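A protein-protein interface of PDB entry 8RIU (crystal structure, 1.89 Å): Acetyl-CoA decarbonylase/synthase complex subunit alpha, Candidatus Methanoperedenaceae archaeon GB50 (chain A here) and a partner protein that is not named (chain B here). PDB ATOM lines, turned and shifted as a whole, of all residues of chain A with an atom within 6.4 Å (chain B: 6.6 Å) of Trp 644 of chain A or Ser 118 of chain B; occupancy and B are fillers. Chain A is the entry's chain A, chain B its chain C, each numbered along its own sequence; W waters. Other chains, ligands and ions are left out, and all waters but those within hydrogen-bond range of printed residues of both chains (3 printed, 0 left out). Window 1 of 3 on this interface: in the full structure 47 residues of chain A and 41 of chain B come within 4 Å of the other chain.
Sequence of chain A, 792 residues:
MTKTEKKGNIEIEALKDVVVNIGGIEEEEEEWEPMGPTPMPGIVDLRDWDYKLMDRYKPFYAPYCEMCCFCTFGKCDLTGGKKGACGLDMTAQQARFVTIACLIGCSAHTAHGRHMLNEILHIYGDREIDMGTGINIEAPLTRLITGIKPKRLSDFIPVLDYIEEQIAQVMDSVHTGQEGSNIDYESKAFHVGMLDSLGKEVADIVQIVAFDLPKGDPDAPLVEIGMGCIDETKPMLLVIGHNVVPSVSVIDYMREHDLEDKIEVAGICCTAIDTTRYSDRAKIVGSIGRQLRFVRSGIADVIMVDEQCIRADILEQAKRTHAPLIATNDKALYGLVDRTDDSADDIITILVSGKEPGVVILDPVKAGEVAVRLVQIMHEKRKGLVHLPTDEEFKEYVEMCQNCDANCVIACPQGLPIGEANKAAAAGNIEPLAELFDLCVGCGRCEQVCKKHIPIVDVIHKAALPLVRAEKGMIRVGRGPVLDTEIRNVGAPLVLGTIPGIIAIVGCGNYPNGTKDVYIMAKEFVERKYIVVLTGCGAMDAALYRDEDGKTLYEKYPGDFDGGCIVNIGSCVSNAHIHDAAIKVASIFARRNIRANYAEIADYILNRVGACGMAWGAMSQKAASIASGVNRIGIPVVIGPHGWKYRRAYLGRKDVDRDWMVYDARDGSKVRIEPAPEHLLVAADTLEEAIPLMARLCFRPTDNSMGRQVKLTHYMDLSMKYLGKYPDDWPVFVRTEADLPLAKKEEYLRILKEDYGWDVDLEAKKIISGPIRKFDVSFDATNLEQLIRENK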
ATOM      1  N   PHE A  60      -0.668 -16.435  13.918  1.00  0.00           N
ATOM      2  CA  PHE A  60      -1.791 -15.903  13.100  1.00  0.00           C
ATOM      3  C   PHE A  60      -1.701 -14.377  13.111  1.00  0.00           C
ATOM      4  O   PHE A  60      -1.463 -13.826  14.181  1.00  0.00           O
ATOM      5  CB  PHE A  60      -3.145 -16.381  13.619  1.00  0.00           C
ATOM      6  CG  PHE A  60      -4.318 -15.590  13.104  1.00  0.00           C
ATOM      7  CD1 PHE A  60      -4.917 -15.917  11.900  1.00  0.00           C
ATOM      8  CD2 PHE A  60      -4.808 -14.508  13.812  1.00  0.00           C
ATOM      9  CE1 PHE A  60      -5.989 -15.184  11.423  1.00  0.00           C
ATOM     10  CE2 PHE A  60      -5.879 -13.774  13.333  1.00  0.00           C
ATOM     11  CZ  PHE A  60      -6.464 -14.113  12.139  1.00  0.00           C
ATOM     12  N   ALA A  62      -3.173 -10.406  12.081  1.00  0.00           N
ATOM     13  CA  ALA A  62      -4.245  -9.471  11.696  1.00  0.00           C
ATOM     14  C   ALA A  62      -3.637  -8.069  11.782  1.00  0.00           C
ATOM     15  O   ALA A  62      -3.710  -7.459  12.842  1.00  0.00           O
ATOM     16  CB  ALA A  62      -5.425  -9.624  12.607  1.00  0.00           C
ATOM     17  N   TYR A  64      -3.515  -4.781  12.346  1.00  0.00           N
ATOM     18  CA  TYR A  64      -4.292  -3.573  12.729  1.00  0.00           C
ATOM     19  C   TYR A  64      -3.739  -2.411  11.911  1.00  0.00           C
ATOM     20  O   TYR A  64      -4.534  -1.638  11.374  1.00  0.00           O
ATOM     21  CB  TYR A  64      -4.196  -3.335  14.234  1.00  0.00           C
ATOM     22  CG  TYR A  64      -5.285  -2.485  14.831  1.00  0.00           C
ATOM     23  CD1 TYR A  64      -6.481  -2.276  14.164  1.00  0.00           C
ATOM     24  CD2 TYR A  64      -5.122  -1.894  16.071  1.00  0.00           C
ATOM     25  CE1 TYR A  64      -7.482  -1.497  14.716  1.00  0.00           C
ATOM     26  CE2 TYR A  64      -6.113  -1.112  16.636  1.00  0.00           C
ATOM     27  CZ  TYR A  64      -7.299  -0.915  15.956  1.00  0.00           C
ATOM     28  OH  TYR A  64      -8.283  -0.139  16.510  1.00  0.00           O
ATOM     29  N   ILE A 639      -7.907 -14.256  25.473  1.00  0.00           N
ATOM     30  CA  ILE A 639      -7.964 -12.789  25.695  1.00  0.00           C
ATOM     31  C   ILE A 639      -9.306 -12.281  25.170  1.00  0.00           C
ATOM     32  O   ILE A 639      -9.998 -13.044  24.510  1.00  0.00           O
ATOM     33  CB  ILE A 639      -6.778 -12.097  25.004  1.00  0.00           C
ATOM     34  CG1 ILE A 639      -6.787 -12.328  23.493  1.00  0.00           C
ATOM     35  CG2 ILE A 639      -5.464 -12.522  25.638  1.00  0.00           C
ATOM     36  CD1 ILE A 639      -5.533 -11.860  22.802  1.00  0.00           C
ATOM     37  N   GLY A 640      -9.644 -11.037  25.477  1.00  0.00           N
ATOM     38  CA  GLY A 640     -10.909 -10.453  25.024  1.00  0.00           C
ATOM     39  C   GLY A 640     -10.859 -10.009  23.573  1.00  0.00           C
ATOM     40  O   GLY A 640      -9.798 -10.086  22.957  1.00  0.00           O
ATOM     41  N   PRO A 641     -11.978  -9.519  23.018  1.00  0.00           N
ATOM     42  CA  PRO A 641     -12.028  -9.146  21.591  1.00  0.00           C
ATOM     43  C   PRO A 641     -11.101  -7.998  21.223  1.00  0.00           C
ATOM     44  O   PRO A 641     -10.683  -7.901  20.063  1.00  0.00           O
ATOM     45  CB  PRO A 641     -13.505  -8.778  21.369  1.00  0.00           C
ATOM     46  CG  PRO A 641     -14.061  -8.497  22.732  1.00  0.00           C
ATOM     47  CD  PRO A 641     -13.255  -9.291  23.716  1.00  0.00           C
ATOM     48  N   HIS A 642     -10.767  -7.118  22.168  1.00  0.00           N
ATOM     49  CA  HIS A 642      -9.768  -6.090  21.898  1.00  0.00           C
ATOM     50  C   HIS A 642      -8.392  -6.692  21.642  1.00  0.00           C
ATOM     51  O   HIS A 642      -7.520  -6.007  21.100  1.00  0.00           O
ATOM     52  CB  HIS A 642      -9.692  -5.117  23.077  1.00  0.00           C
ATOM     53  CG  HIS A 642     -10.877  -4.212  23.194  1.00  0.00           C
ATOM     54  ND1 HIS A 642     -11.085  -3.146  22.347  1.00  0.00           N
ATOM     55  CD2 HIS A 642     -11.925  -4.222  24.052  1.00  0.00           C
ATOM     56  CE1 HIS A 642     -12.205  -2.532  22.683  1.00  0.00           C
ATOM     57  NE2 HIS A 642     -12.735  -3.163  23.715  1.00  0.00           N
ATOM     58  N   GLY A 643      -8.178  -7.957  22.022  1.00  0.00           N
ATOM     59  CA  GLY A 643      -6.871  -8.582  21.883  1.00  0.00           C
ATOM     60  C   GLY A 643      -6.439  -8.811  20.449  1.00  0.00           C
ATOM     61  O   GLY A 643      -5.246  -9.016  20.196  1.00  0.00           O
ATOM     62  N   TRP A 644      -7.382  -8.787  19.503  1.00  0.00           N
ATOM     63  CA  TRP A 644      -7.002  -8.777  18.099  1.00  0.00           C
ATOM     64  C   TRP A 644      -6.068  -7.621  17.779  1.00  0.00           C
ATOM     65  O   TRP A 644      -5.351  -7.681  16.779  1.00  0.00           O
ATOM     66  CB  TRP A 644      -8.221  -8.649  17.190  1.00  0.00           C
ATOM     67  CG  TRP A 644      -9.142  -9.817  17.108  1.00  0.00           C
ATOM     68  CD1 TRP A 644     -10.038 -10.228  18.047  1.00  0.00           C
ATOM     69  CD2 TRP A 644      -9.287 -10.704  15.995  1.00  0.00           C
ATOM     70  NE1 TRP A 644     -10.734 -11.328  17.588  1.00  0.00           N
ATOM     71  CE2 TRP A 644     -10.288 -11.638  16.329  1.00  0.00           C
ATOM     72  CE3 TRP A 644      -8.658 -10.803  14.744  1.00  0.00           C
ATOM     73  CZ2 TRP A 644     -10.678 -12.656  15.462  1.00  0.00           C
ATOM     74  CZ3 TRP A 644      -9.048 -11.811  13.881  1.00  0.00           C
ATOM     75  CH2 TRP A 644     -10.055 -12.724  14.243  1.00  0.00           C
ATOM     76  N   LYS A 645      -6.091  -6.557  18.583  1.00  0.00           N
ATOM     77  CA  LYS A 645      -5.285  -5.378  18.291  1.00  0.00           C
ATOM     78  C   LYS A 645      -3.803  -5.602  18.562  1.00  0.00           C
ATOM     79  O   LYS A 645      -2.980  -4.801  18.102  1.00  0.00           O
ATOM     80  CB  LYS A 645      -5.815  -4.196  19.101  1.00  0.00           C
ATOM     81  CG  LYS A 645      -7.282  -3.886  18.808  1.00  0.00           C
ATOM     82  CD  LYS A 645      -7.807  -2.722  19.634  1.00  0.00           C
ATOM     83  CE  LYS A 645      -9.303  -2.506  19.398  1.00  0.00           C
ATOM     84  NZ  LYS A 645      -9.842  -1.405  20.230  1.00  0.00           N
ATOM     85  N   TYR A 646      -3.441  -6.656  19.296  1.00  0.00           N
ATOM     86  CA  TYR A 646      -2.047  -7.072  19.388  1.00  0.00           C
ATOM     87  C   TYR A 646      -1.529  -7.627  18.065  1.00  0.00           C
ATOM     88  O   TYR A 646      -0.322  -7.858  17.941  1.00  0.00           O
ATOM     89  CB  TYR A 646      -1.871  -8.136  20.478  1.00  0.00           C
ATOM     90  CG  TYR A 646      -1.968  -7.638  21.914  1.00  0.00           C
ATOM     91  CD1 TYR A 646      -1.213  -6.563  22.365  1.00  0.00           C
ATOM     92  CD2 TYR A 646      -2.833  -8.247  22.810  1.00  0.00           C
ATOM     93  CE1 TYR A 646      -1.313  -6.119  23.681  1.00  0.00           C
ATOM     94  CE2 TYR A 646      -2.941  -7.815  24.111  1.00  0.00           C
ATOM     95  CZ  TYR A 646      -2.176  -6.752  24.548  1.00  0.00           C
ATOM     96  OH  TYR A 646      -2.298  -6.329  25.856  1.00  0.00           O
ATOM     97  N   ARG A 647      -2.431  -7.839  17.105  1.00  0.00           N
ATOM     98  CA  ARG A 647      -2.055  -8.291  15.733  1.00  0.00           C
ATOM     99  C   ARG A 647      -1.770  -9.799  15.690  1.00  0.00           C
ATOM    100  O   ARG A 647      -2.264 -10.445  14.771  1.00  0.00           O
ATOM    101  CB  ARG A 647      -0.898  -7.454  15.182  1.00  0.00           C
ATOM    102  CG  ARG A 647      -1.120  -5.950  15.217  1.00  0.00           C
ATOM    103  CD  ARG A 647      -0.054  -5.296  14.367  1.00  0.00           C
ATOM    104  NE  ARG A 647       0.112  -3.877  14.620  1.00  0.00           N
ATOM    105  CZ  ARG A 647       1.008  -3.120  14.005  1.00  0.00           C
ATOM    106  NH1 ARG A 647       1.721  -3.623  13.013  1.00  0.00           N
ATOM    107  NH2 ARG A 647       1.192  -1.869  14.384  1.00  0.00           N
ATOM    108  N   ARG A 648      -1.009 -10.334  16.647  1.00  0.00           N
ATOM    109  CA  ARG A 648      -0.594 -11.761  16.537  1.00  0.00           C
ATOM    110  C   ARG A 648      -1.270 -12.679  17.558  1.00  0.00           C
ATOM    111  O   ARG A 648      -1.443 -12.258  18.712  1.00  0.00           O
ATOM    112  CB  ARG A 648       0.927 -11.890  16.683  1.00  0.00           C
ATOM    113  CG  ARG A 648       1.451 -13.314  16.560  1.00  0.00           C
ATOM    114  CD  ARG A 648       1.471 -14.067  17.878  1.00  0.00           C
ATOM    115  NE  ARG A 648       2.515 -13.612  18.783  1.00  0.00           N
ATOM    116  CZ  ARG A 648       2.298 -13.061  19.971  1.00  0.00           C
ATOM    117  NH1 ARG A 648       1.082 -12.673  20.312  1.00  0.00           N
ATOM    118  NH2 ARG A 648       3.301 -12.899  20.817  1.00  0.00           N
ATOM    119  N   ALA A 683      -8.355 -15.044  21.038  1.00  0.00           N
ATOM    120  CA  ALA A 683      -9.279 -14.001  21.469  1.00  0.00           C
ATOM    121  C   ALA A 683     -10.717 -14.451  21.253  1.00  0.00           C
ATOM    122  O   ALA A 683     -11.094 -14.849  20.144  1.00  0.00           O
ATOM    123  CB  ALA A 683      -9.031 -12.700  20.707  1.00  0.00           C
ATOM    124  N   ALA A 684     -11.520 -14.302  22.308  1.00  0.00           N
ATOM    125  CA  ALA A 684     -12.963 -14.605  22.219  1.00  0.00           C
ATOM    126  C   ALA A 684     -13.750 -13.290  22.273  1.00  0.00           C
ATOM    127  O   ALA A 684     -13.197 -12.305  22.771  1.00  0.00           O
ATOM    128  CB  ALA A 684     -13.356 -15.554  23.314  1.00  0.00           C
ATOM    129  N   ASP A 685     -15.006 -13.300  21.834  1.00  0.00           N
ATOM    130  CA  ASP A 685     -15.781 -12.044  21.715  1.00  0.00           C
ATOM    131  C   ASP A 685     -16.716 -11.809  22.897  1.00  0.00           C
ATOM    132  O   ASP A 685     -16.901 -10.659  23.264  1.00  0.00           O
ATOM    133  CB  ASP A 685     -16.616 -12.081  20.440  1.00  0.00           C
ATOM    134  CG  ASP A 685     -15.802 -11.844  19.184  1.00  0.00           C
ATOM    135  OD1 ASP A 685     -15.361 -10.707  18.993  1.00  0.00           O
ATOM    136  OD2 ASP A 685     -15.611 -12.802  18.421  1.00  0.00           O
ATOM    137  N   GLY B  84     -15.203 -20.053  16.755  1.00  0.00           N
ATOM    138  CA  GLY B  84     -14.650 -18.745  17.126  1.00  0.00           C
ATOM    139  C   GLY B  84     -14.281 -17.918  15.909  1.00  0.00           C
ATOM    140  O   GLY B  84     -13.828 -18.493  14.923  1.00  0.00           O
ATOM    141  N   LEU B  85     -14.505 -16.605  15.989  1.00  0.00           N
ATOM    142  CA  LEU B  85     -14.114 -15.700  14.881  1.00  0.00           C
ATOM    143  C   LEU B  85     -12.611 -15.856  14.655  1.00  0.00           C
ATOM    144  O   LEU B  85     -12.202 -15.938  13.482  1.00  0.00           O
ATOM    145  CB  LEU B  85     -14.456 -14.264  15.287  1.00  0.00           C
ATOM    146  CG  LEU B  85     -14.378 -13.226  14.169  1.00  0.00           C
ATOM    147  CD1 LEU B  85     -15.538 -13.394  13.200  1.00  0.00           C
ATOM    148  CD2 LEU B  85     -14.361 -11.817  14.743  1.00  0.00           C
ATOM    149  N   HIS B  86     -11.839 -15.924  15.744  1.00  0.00           N
ATOM    150  CA  HIS B  86     -10.357 -16.008  15.634  1.00  0.00           C
ATOM    151  C   HIS B  86      -9.959 -17.249  14.832  1.00  0.00           C
ATOM    152  O   HIS B  86      -9.250 -17.070  13.843  1.00  0.00           O
ATOM    153  CB  HIS B  86      -9.693 -15.979  17.015  1.00  0.00           C
ATOM    154  CG  HIS B  86      -8.506 -15.078  17.056  1.00  0.00           C
ATOM    155  ND1 HIS B  86      -7.905 -14.658  18.221  1.00  0.00           N
ATOM    156  CD2 HIS B  86      -7.814 -14.514  16.059  1.00  0.00           C
ATOM    157  CE1 HIS B  86      -6.887 -13.866  17.926  1.00  0.00           C
ATOM    158  NE2 HIS B  86      -6.812 -13.766  16.618  1.00  0.00           N
ATOM    159  N   GLU B  87     -10.383 -18.442  15.255  1.00  0.00           N
ATOM    160  CA  GLU B  87      -9.966 -19.687  14.555  1.00  0.00           C
ATOM    161  C   GLU B  87     -10.540 -19.678  13.134  1.00  0.00           C
ATOM    162  O   GLU B  87      -9.856 -20.173  12.220  1.00  0.00           O
ATOM    163  CB  GLU B  87     -10.407 -20.926  15.339  1.00  0.00           C
ATOM    164  CG  GLU B  87     -11.885 -20.948  15.680  1.00  0.00           C
ATOM    165  CD  GLU B  87     -12.311 -22.128  16.538  1.00  0.00           C
ATOM    166  OE1 GLU B  87     -11.454 -22.984  16.828  1.00  0.00           O
ATOM    167  OE2 GLU B  87     -13.497 -22.186  16.913  1.00  0.00           O
ATOM    168  N   ALA B  89     -10.928 -17.161  11.113  1.00  0.00           N
ATOM    169  CA  ALA B  89     -10.006 -16.374  10.263  1.00  0.00           C
ATOM    170  C   ALA B  89      -8.812 -17.245   9.866  1.00  0.00           C
ATOM    171  O   ALA B  89      -8.473 -17.277   8.689  1.00  0.00           O
ATOM    172  CB  ALA B  89      -9.559 -15.144  10.989  1.00  0.00           C
ATOM    173  N   ASN B  90      -8.187 -17.906  10.843  1.00  0.00           N
ATOM    174  CA  ASN B  90      -6.972 -18.719  10.567  1.00  0.00           C
ATOM    175  C   ASN B  90      -7.320 -19.830   9.577  1.00  0.00           C
ATOM    176  O   ASN B  90      -6.490 -20.132   8.708  1.00  0.00           O
ATOM    177  CB  ASN B  90      -6.386 -19.297  11.855  1.00  0.00           C
ATOM    178  CG  ASN B  90      -5.087 -20.044  11.641  1.00  0.00           C
ATOM    179  OD1 ASN B  90      -4.093 -19.459  11.217  1.00  0.00           O
ATOM    180  ND2 ASN B  90      -5.085 -21.332  11.938  1.00  0.00           N
ATOM    181  N   GLY B 114     -21.693  -8.357  13.914  1.00  0.00           N
ATOM    182  CA  GLY B 114     -20.476  -8.665  14.645  1.00  0.00           C
ATOM    183  C   GLY B 114     -19.972  -7.466  15.428  1.00  0.00           C
ATOM    184  O   GLY B 114     -20.181  -6.320  15.038  1.00  0.00           O
ATOM    185  N   ILE B 115     -19.302  -7.741  16.552  1.00  0.00           N
ATOM    186  CA  ILE B 115     -18.633  -6.677  17.289  1.00  0.00           C
ATOM    187  C   ILE B 115     -17.629  -6.004  16.366  1.00  0.00           C
ATOM    188  O   ILE B 115     -16.807  -6.671  15.728  1.00  0.00           O
ATOM    189  CB  ILE B 115     -17.961  -7.243  18.548  1.00  0.00           C
ATOM    190  CG1 ILE B 115     -19.018  -7.696  19.561  1.00  0.00           C
ATOM    191  CG2 ILE B 115     -17.006  -6.217  19.170  1.00  0.00           C
ATOM    192  CD1 ILE B 115     -18.442  -8.421  20.772  1.00  0.00           C
ATOM    193  N   TYR B 116     -17.671  -4.670  16.301  1.00  0.00           N
ATOM    194  CA  TYR B 116     -16.969  -3.967  15.228  1.00  0.00           C
ATOM    195  C   TYR B 116     -15.477  -4.267  15.227  1.00  0.00           C
ATOM    196  O   TYR B 116     -14.915  -4.686  14.210  1.00  0.00           O
ATOM    197  CB  TYR B 116     -17.161  -2.455  15.336  1.00  0.00           C
ATOM    198  CG  TYR B 116     -16.381  -1.727  14.261  1.00  0.00           C
ATOM    199  CD1 TYR B 116     -16.798  -1.761  12.934  1.00  0.00           C
ATOM    200  CD2 TYR B 116     -15.197  -1.060  14.558  1.00  0.00           C
ATOM    201  CE1 TYR B 116     -16.091  -1.115  11.945  1.00  0.00           C
ATOM    202  CE2 TYR B 116     -14.475  -0.403  13.570  1.00  0.00           C
ATOM    203  CZ  TYR B 116     -14.926  -0.436  12.267  1.00  0.00           C
ATOM    204  OH  TYR B 116     -14.221   0.206  11.276  1.00  0.00           O
ATOM    205  N   TYR B 117     -14.802  -3.995  16.348  1.00  0.00           N
ATOM    206  CA  TYR B 117     -13.344  -3.980  16.325  1.00  0.00           C
ATOM    207  C   TYR B 117     -12.754  -5.379  16.179  1.00  0.00           C
ATOM    208  O   TYR B 117     -11.647  -5.522  15.646  1.00  0.00           O
ATOM    209  CB  TYR B 117     -12.793  -3.294  17.578  1.00  0.00           C
ATOM    210  CG  TYR B 117     -13.472  -3.690  18.875  1.00  0.00           C
ATOM    211  CD1 TYR B 117     -13.005  -4.759  19.630  1.00  0.00           C
ATOM    212  CD2 TYR B 117     -14.560  -2.981  19.356  1.00  0.00           C
ATOM    213  CE1 TYR B 117     -13.616  -5.119  20.802  1.00  0.00           C
ATOM    214  CE2 TYR B 117     -15.181  -3.339  20.528  1.00  0.00           C
ATOM    215  CZ  TYR B 117     -14.704  -4.407  21.250  1.00  0.00           C
ATOM    216  OH  TYR B 117     -15.321  -4.775  22.424  1.00  0.00           O
ATOM    217  N   SER B 118     -13.458  -6.416  16.644  1.00  0.00           N
ATOM    218  CA  SER B 118     -12.985  -7.777  16.392  1.00  0.00           C
ATOM    219  C   SER B 118     -13.321  -8.216  14.974  1.00  0.00           C
ATOM    220  O   SER B 118     -12.473  -8.787  14.276  1.00  0.00           O
ATOM    221  CB  SER B 118     -13.578  -8.762  17.408  1.00  0.00           C
ATOM    222  OG  SER B 118     -14.991  -8.665  17.476  1.00  0.00           O
ATOM    223  N   THR B 119     -14.546  -7.943  14.520  1.00  0.00           N
ATOM    224  CA  THR B 119     -14.897  -8.274  13.146  1.00  0.00           C
ATOM    225  C   THR B 119     -13.967  -7.579  12.162  1.00  0.00           C
ATOM    226  O   THR B 119     -13.553  -8.178  11.165  1.00  0.00           O
ATOM    227  CB  THR B 119     -16.349  -7.901  12.859  1.00  0.00           C
ATOM    228  OG1 THR B 119     -17.209  -8.520  13.829  1.00  0.00           O
ATOM    229  CG2 THR B 119     -16.744  -8.362  11.455  1.00  0.00           C
ATOM    230  N   SER B 120     -13.630  -6.311  12.419  1.00  0.00           N
ATOM    231  CA  SER B 120     -12.736  -5.596  11.513  1.00  0.00           C
ATOM    232  C   SER B 120     -11.396  -6.313  11.401  1.00  0.00           C
ATOM    233  O   SER B 120     -10.882  -6.530  10.299  1.00  0.00           O
ATOM    234  CB  SER B 120     -12.536  -4.157  11.984  1.00  0.00           C
ATOM    235  OG  SER B 120     -11.661  -3.459  11.110  1.00  0.00           O
ATOM    236  N   GLN B 121     -10.822  -6.705  12.537  1.00  0.00           N
ATOM    237  CA  GLN B 121      -9.551  -7.422  12.511  1.00  0.00           C
ATOM    238  C   GLN B 121      -9.686  -8.788  11.843  1.00  0.00           C
ATOM    239  O   GLN B 121      -8.740  -9.271  11.206  1.00  0.00           O
ATOM    240  CB  GLN B 121      -9.026  -7.563  13.932  1.00  0.00           C
ATOM    241  CG  GLN B 121      -8.430  -6.275  14.468  1.00  0.00           C
ATOM    242  CD  GLN B 121      -7.185  -5.894  13.709  1.00  0.00           C
ATOM    243  OE1 GLN B 121      -7.239  -5.146  12.725  1.00  0.00           O
ATOM    244  NE2 GLN B 121      -6.055  -6.437  14.136  1.00  0.00           N
ATOM    245  N   PHE B 122     -10.850  -9.416  11.970  1.00  0.00           N
ATOM    246  CA  PHE B 122     -11.123 -10.639  11.223  1.00  0.00           C
ATOM    247  C   PHE B 122     -11.090 -10.358   9.727  1.00  0.00           C
ATOM    248  O   PHE B 122     -10.447 -11.088   8.959  1.00  0.00           O
ATOM    249  CB  PHE B 122     -12.473 -11.197  11.697  1.00  0.00           C
ATOM    250  CG  PHE B 122     -13.087 -12.235  10.790  1.00  0.00           C
ATOM    251  CD1 PHE B 122     -13.925 -11.861   9.748  1.00  0.00           C
ATOM    252  CD2 PHE B 122     -12.847 -13.585  11.000  1.00  0.00           C
ATOM    253  CE1 PHE B 122     -14.505 -12.813   8.924  1.00  0.00           C
ATOM    254  CE2 PHE B 122     -13.420 -14.543  10.177  1.00  0.00           C
ATOM    255  CZ  PHE B 122     -14.247 -14.156   9.135  1.00  0.00           C
ATOM    256  N   LEU B 123     -11.670  -9.242   9.305  1.00  0.00           N
ATOM    257  CA  LEU B 123     -11.631  -8.860   7.870  1.00  0.00           C
ATOM    258  C   LEU B 123     -10.195  -8.528   7.430  1.00  0.00           C
ATOM    259  O   LEU B 123      -9.804  -8.969   6.352  1.00  0.00           O
ATOM    260  CB  LEU B 123     -12.570  -7.671   7.670  1.00  0.00           C
ATOM    261  CG  LEU B 123     -14.056  -7.966   7.857  1.00  0.00           C
ATOM    262  CD1 LEU B 123     -14.855  -6.680   7.961  1.00  0.00           C
ATOM    263  CD2 LEU B 123     -14.584  -8.830   6.724  1.00  0.00           C
ATOM    264  N   ILE B 124      -9.452  -7.774   8.236  1.00  0.00           N
ATOM    265  CA  ILE B 124      -8.070  -7.360   7.855  1.00  0.00           C
ATOM    266  C   ILE B 124      -7.212  -8.610   7.663  1.00  0.00           C
ATOM    267  O   ILE B 124      -6.390  -8.613   6.753  1.00  0.00           O
ATOM    268  CB  ILE B 124      -7.453  -6.385   8.880  1.00  0.00           C
ATOM    269  CG1 ILE B 124      -6.704  -5.253   8.174  1.00  0.00           C
ATOM    270  CG2 ILE B 124      -6.563  -7.105   9.875  1.00  0.00           C
ATOM    271  CD1 ILE B 124      -7.228  -3.879   8.486  1.00  0.00           C
ATOM    272  N   SER B 125      -7.430  -9.626   8.489  1.00  0.00           N
ATOM    273  CA  SER B 125      -6.659 -10.886   8.408  1.00  0.00           C
ATOM    274  C   SER B 125      -6.859 -11.495   7.026  1.00  0.00           C
ATOM    275  O   SER B 125      -5.870 -11.818   6.376  1.00  0.00           O
ATOM    276  CB  SER B 125      -7.083 -11.836   9.490  1.00  0.00           C
ATOM    277  OG  SER B 125      -8.336 -12.428   9.206  1.00  0.00           O
ATOM    278  N   HIS B 145     -16.980  -1.005   7.090  1.00  0.00           N
ATOM    279  CA  HIS B 145     -15.801  -1.872   7.357  1.00  0.00           C
ATOM    280  C   HIS B 145     -14.682  -1.514   6.373  1.00  0.00           C
ATOM    281  O   HIS B 145     -14.619  -2.103   5.273  1.00  0.00           O
ATOM    282  CB  HIS B 145     -16.204  -3.350   7.339  1.00  0.00           C
ATOM    283  CG  HIS B 145     -16.615  -3.859   8.681  1.00  0.00           C
ATOM    284  ND1 HIS B 145     -15.760  -3.893   9.760  1.00  0.00           N
ATOM    285  CD2 HIS B 145     -17.782  -4.345   9.118  1.00  0.00           C
ATOM    286  CE1 HIS B 145     -16.398  -4.391  10.809  1.00  0.00           C
ATOM    287  NE2 HIS B 145     -17.627  -4.669  10.440  1.00  0.00           N
HETATM  288  O   HOH W   1      -4.714 -11.735  16.062  1.00  0.00           O
HETATM  289  O   HOH W   2     -12.824 -16.501  18.726  1.00  0.00           O
HETATM  290  O   HOH W   3     -16.081 -15.607  18.244  1.00  0.00           O
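Of the 16 printed residues of chain A, 8 touch a printed residue of chain B.
Hydrophobic or aromatic side chains of chain A within 4 Å of the printed part of chain B: Phe 60, Ala 62, Tyr 64, Pro 641, His 642, Trp 644 and Ala 683.
Among the printed residues, no Asp or Glu carboxylate lies within 4 Å of a Lys or Arg side-chain nitrogen of the other chain.
Among the printed residues, pairs that only touch across the chains: Tyr 64 of chain A with Gln 121 of chain B (3.3 Å), Trp 644 of chain A with His 86 of chain B (3.4 Å), Phe 60 of chain A with His 86 of chain B (3.4 Å), Phe 60 of chain A with Ala 89 of chain B (3.5 Å), Phe 60 of chain A with Asn 90 of chain B (3.5 Å), Phe 60 of chain A with Ser 125 of chain B (3.5 Å), Trp 644 of chain A with Phe 122 of chain B (3.6 Å), Ala 62 of chain A with Ile 124 of chain B (3.6 Å), Asp 685 of chain A with Leu 85 of chain B (3.6 Å), Asp 685 of chain A with Ile 115 of chain B (3.7 Å), Pro 641 of chain A with Tyr 117 of chain B (3.7 Å), Trp 644 of chain A with Leu 85 of chain B (3.8 Å), Trp 644 of chain A with Ser 118 of chain B (3.8 Å) and Pro 641 of chain A with Ser 118 of chain B (3.96 Å).
O of Trp 644 of chain A lies within hydrogen-bond range of NE2 of Gln 121 of chain B (3.0 Å).
The side-chain carboxylate of Asp 685 of chain A sits at hydrogen-bond distance from the side-chain hydroxyl of Ser 118 of chain B.
O of Ala 62 of chain A is in hydrogen-bond range of NE2 of Gln 121 of chain B.
NE2 of His 642 of chain A sits at hydrogen-bond distance from OH of Tyr 117 of chain B (3.3 Å).
A ring nitrogen (ND1) of His 86 of chain B is in hydrogen-bond range of the backbone NH (N) of Ala 683 of chain A.
The backbone carbonyl oxygen (O) of Ile 115 of chain B sits at hydrogen-bond distance from the side-chain hydroxyl (OG) of Ser 118 of chain B, 3.2 Å away.
The backbone carbonyl oxygen (O) of Arg 647 of chain A sits at hydrogen-bond distance from the backbone NH (N) of Ala 62 of chain A (2.8 Å).
Water W3 bridges the side-chain carboxylate of Asp 685 of chain A and the backbone NH of Leu 85 of chain B.
Water W1 lies within hydrogen-bond range of a ring nitrogen (NE2) of His 86 of chain B (3.0 Å) and the backbone carbonyl oxygen (O) of Arg 647 of chain A (3.1 Å).
Trp 644 of chain A touches just these residues of chain B: Leu 85 (3.8 Å), His 86 (3.4 Å), Ser 118 (3.8 Å), Gln 121 (3.0 Å) and Phe 122 (3.6 Å).
Glu 87 of chain B touches none of the printed residues of chain A.
Printed residues of chain A within 4 Å of Ile 115 of chain B: Asp 685 (3.7 Å).
Of chain A, only Pro 641 (3.96 Å), Trp 644 (3.8 Å) and Asp 685 (2.6 Å) come within 4 Å of Ser 118 of chain B.
Of the printed residues of chain A, Ile 124 of chain B touches Ala 62 (3.6 Å).
The nearest residue of chain A that does not touch Ser 118 of chain B is His 642 of chain A (5.8 Å).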
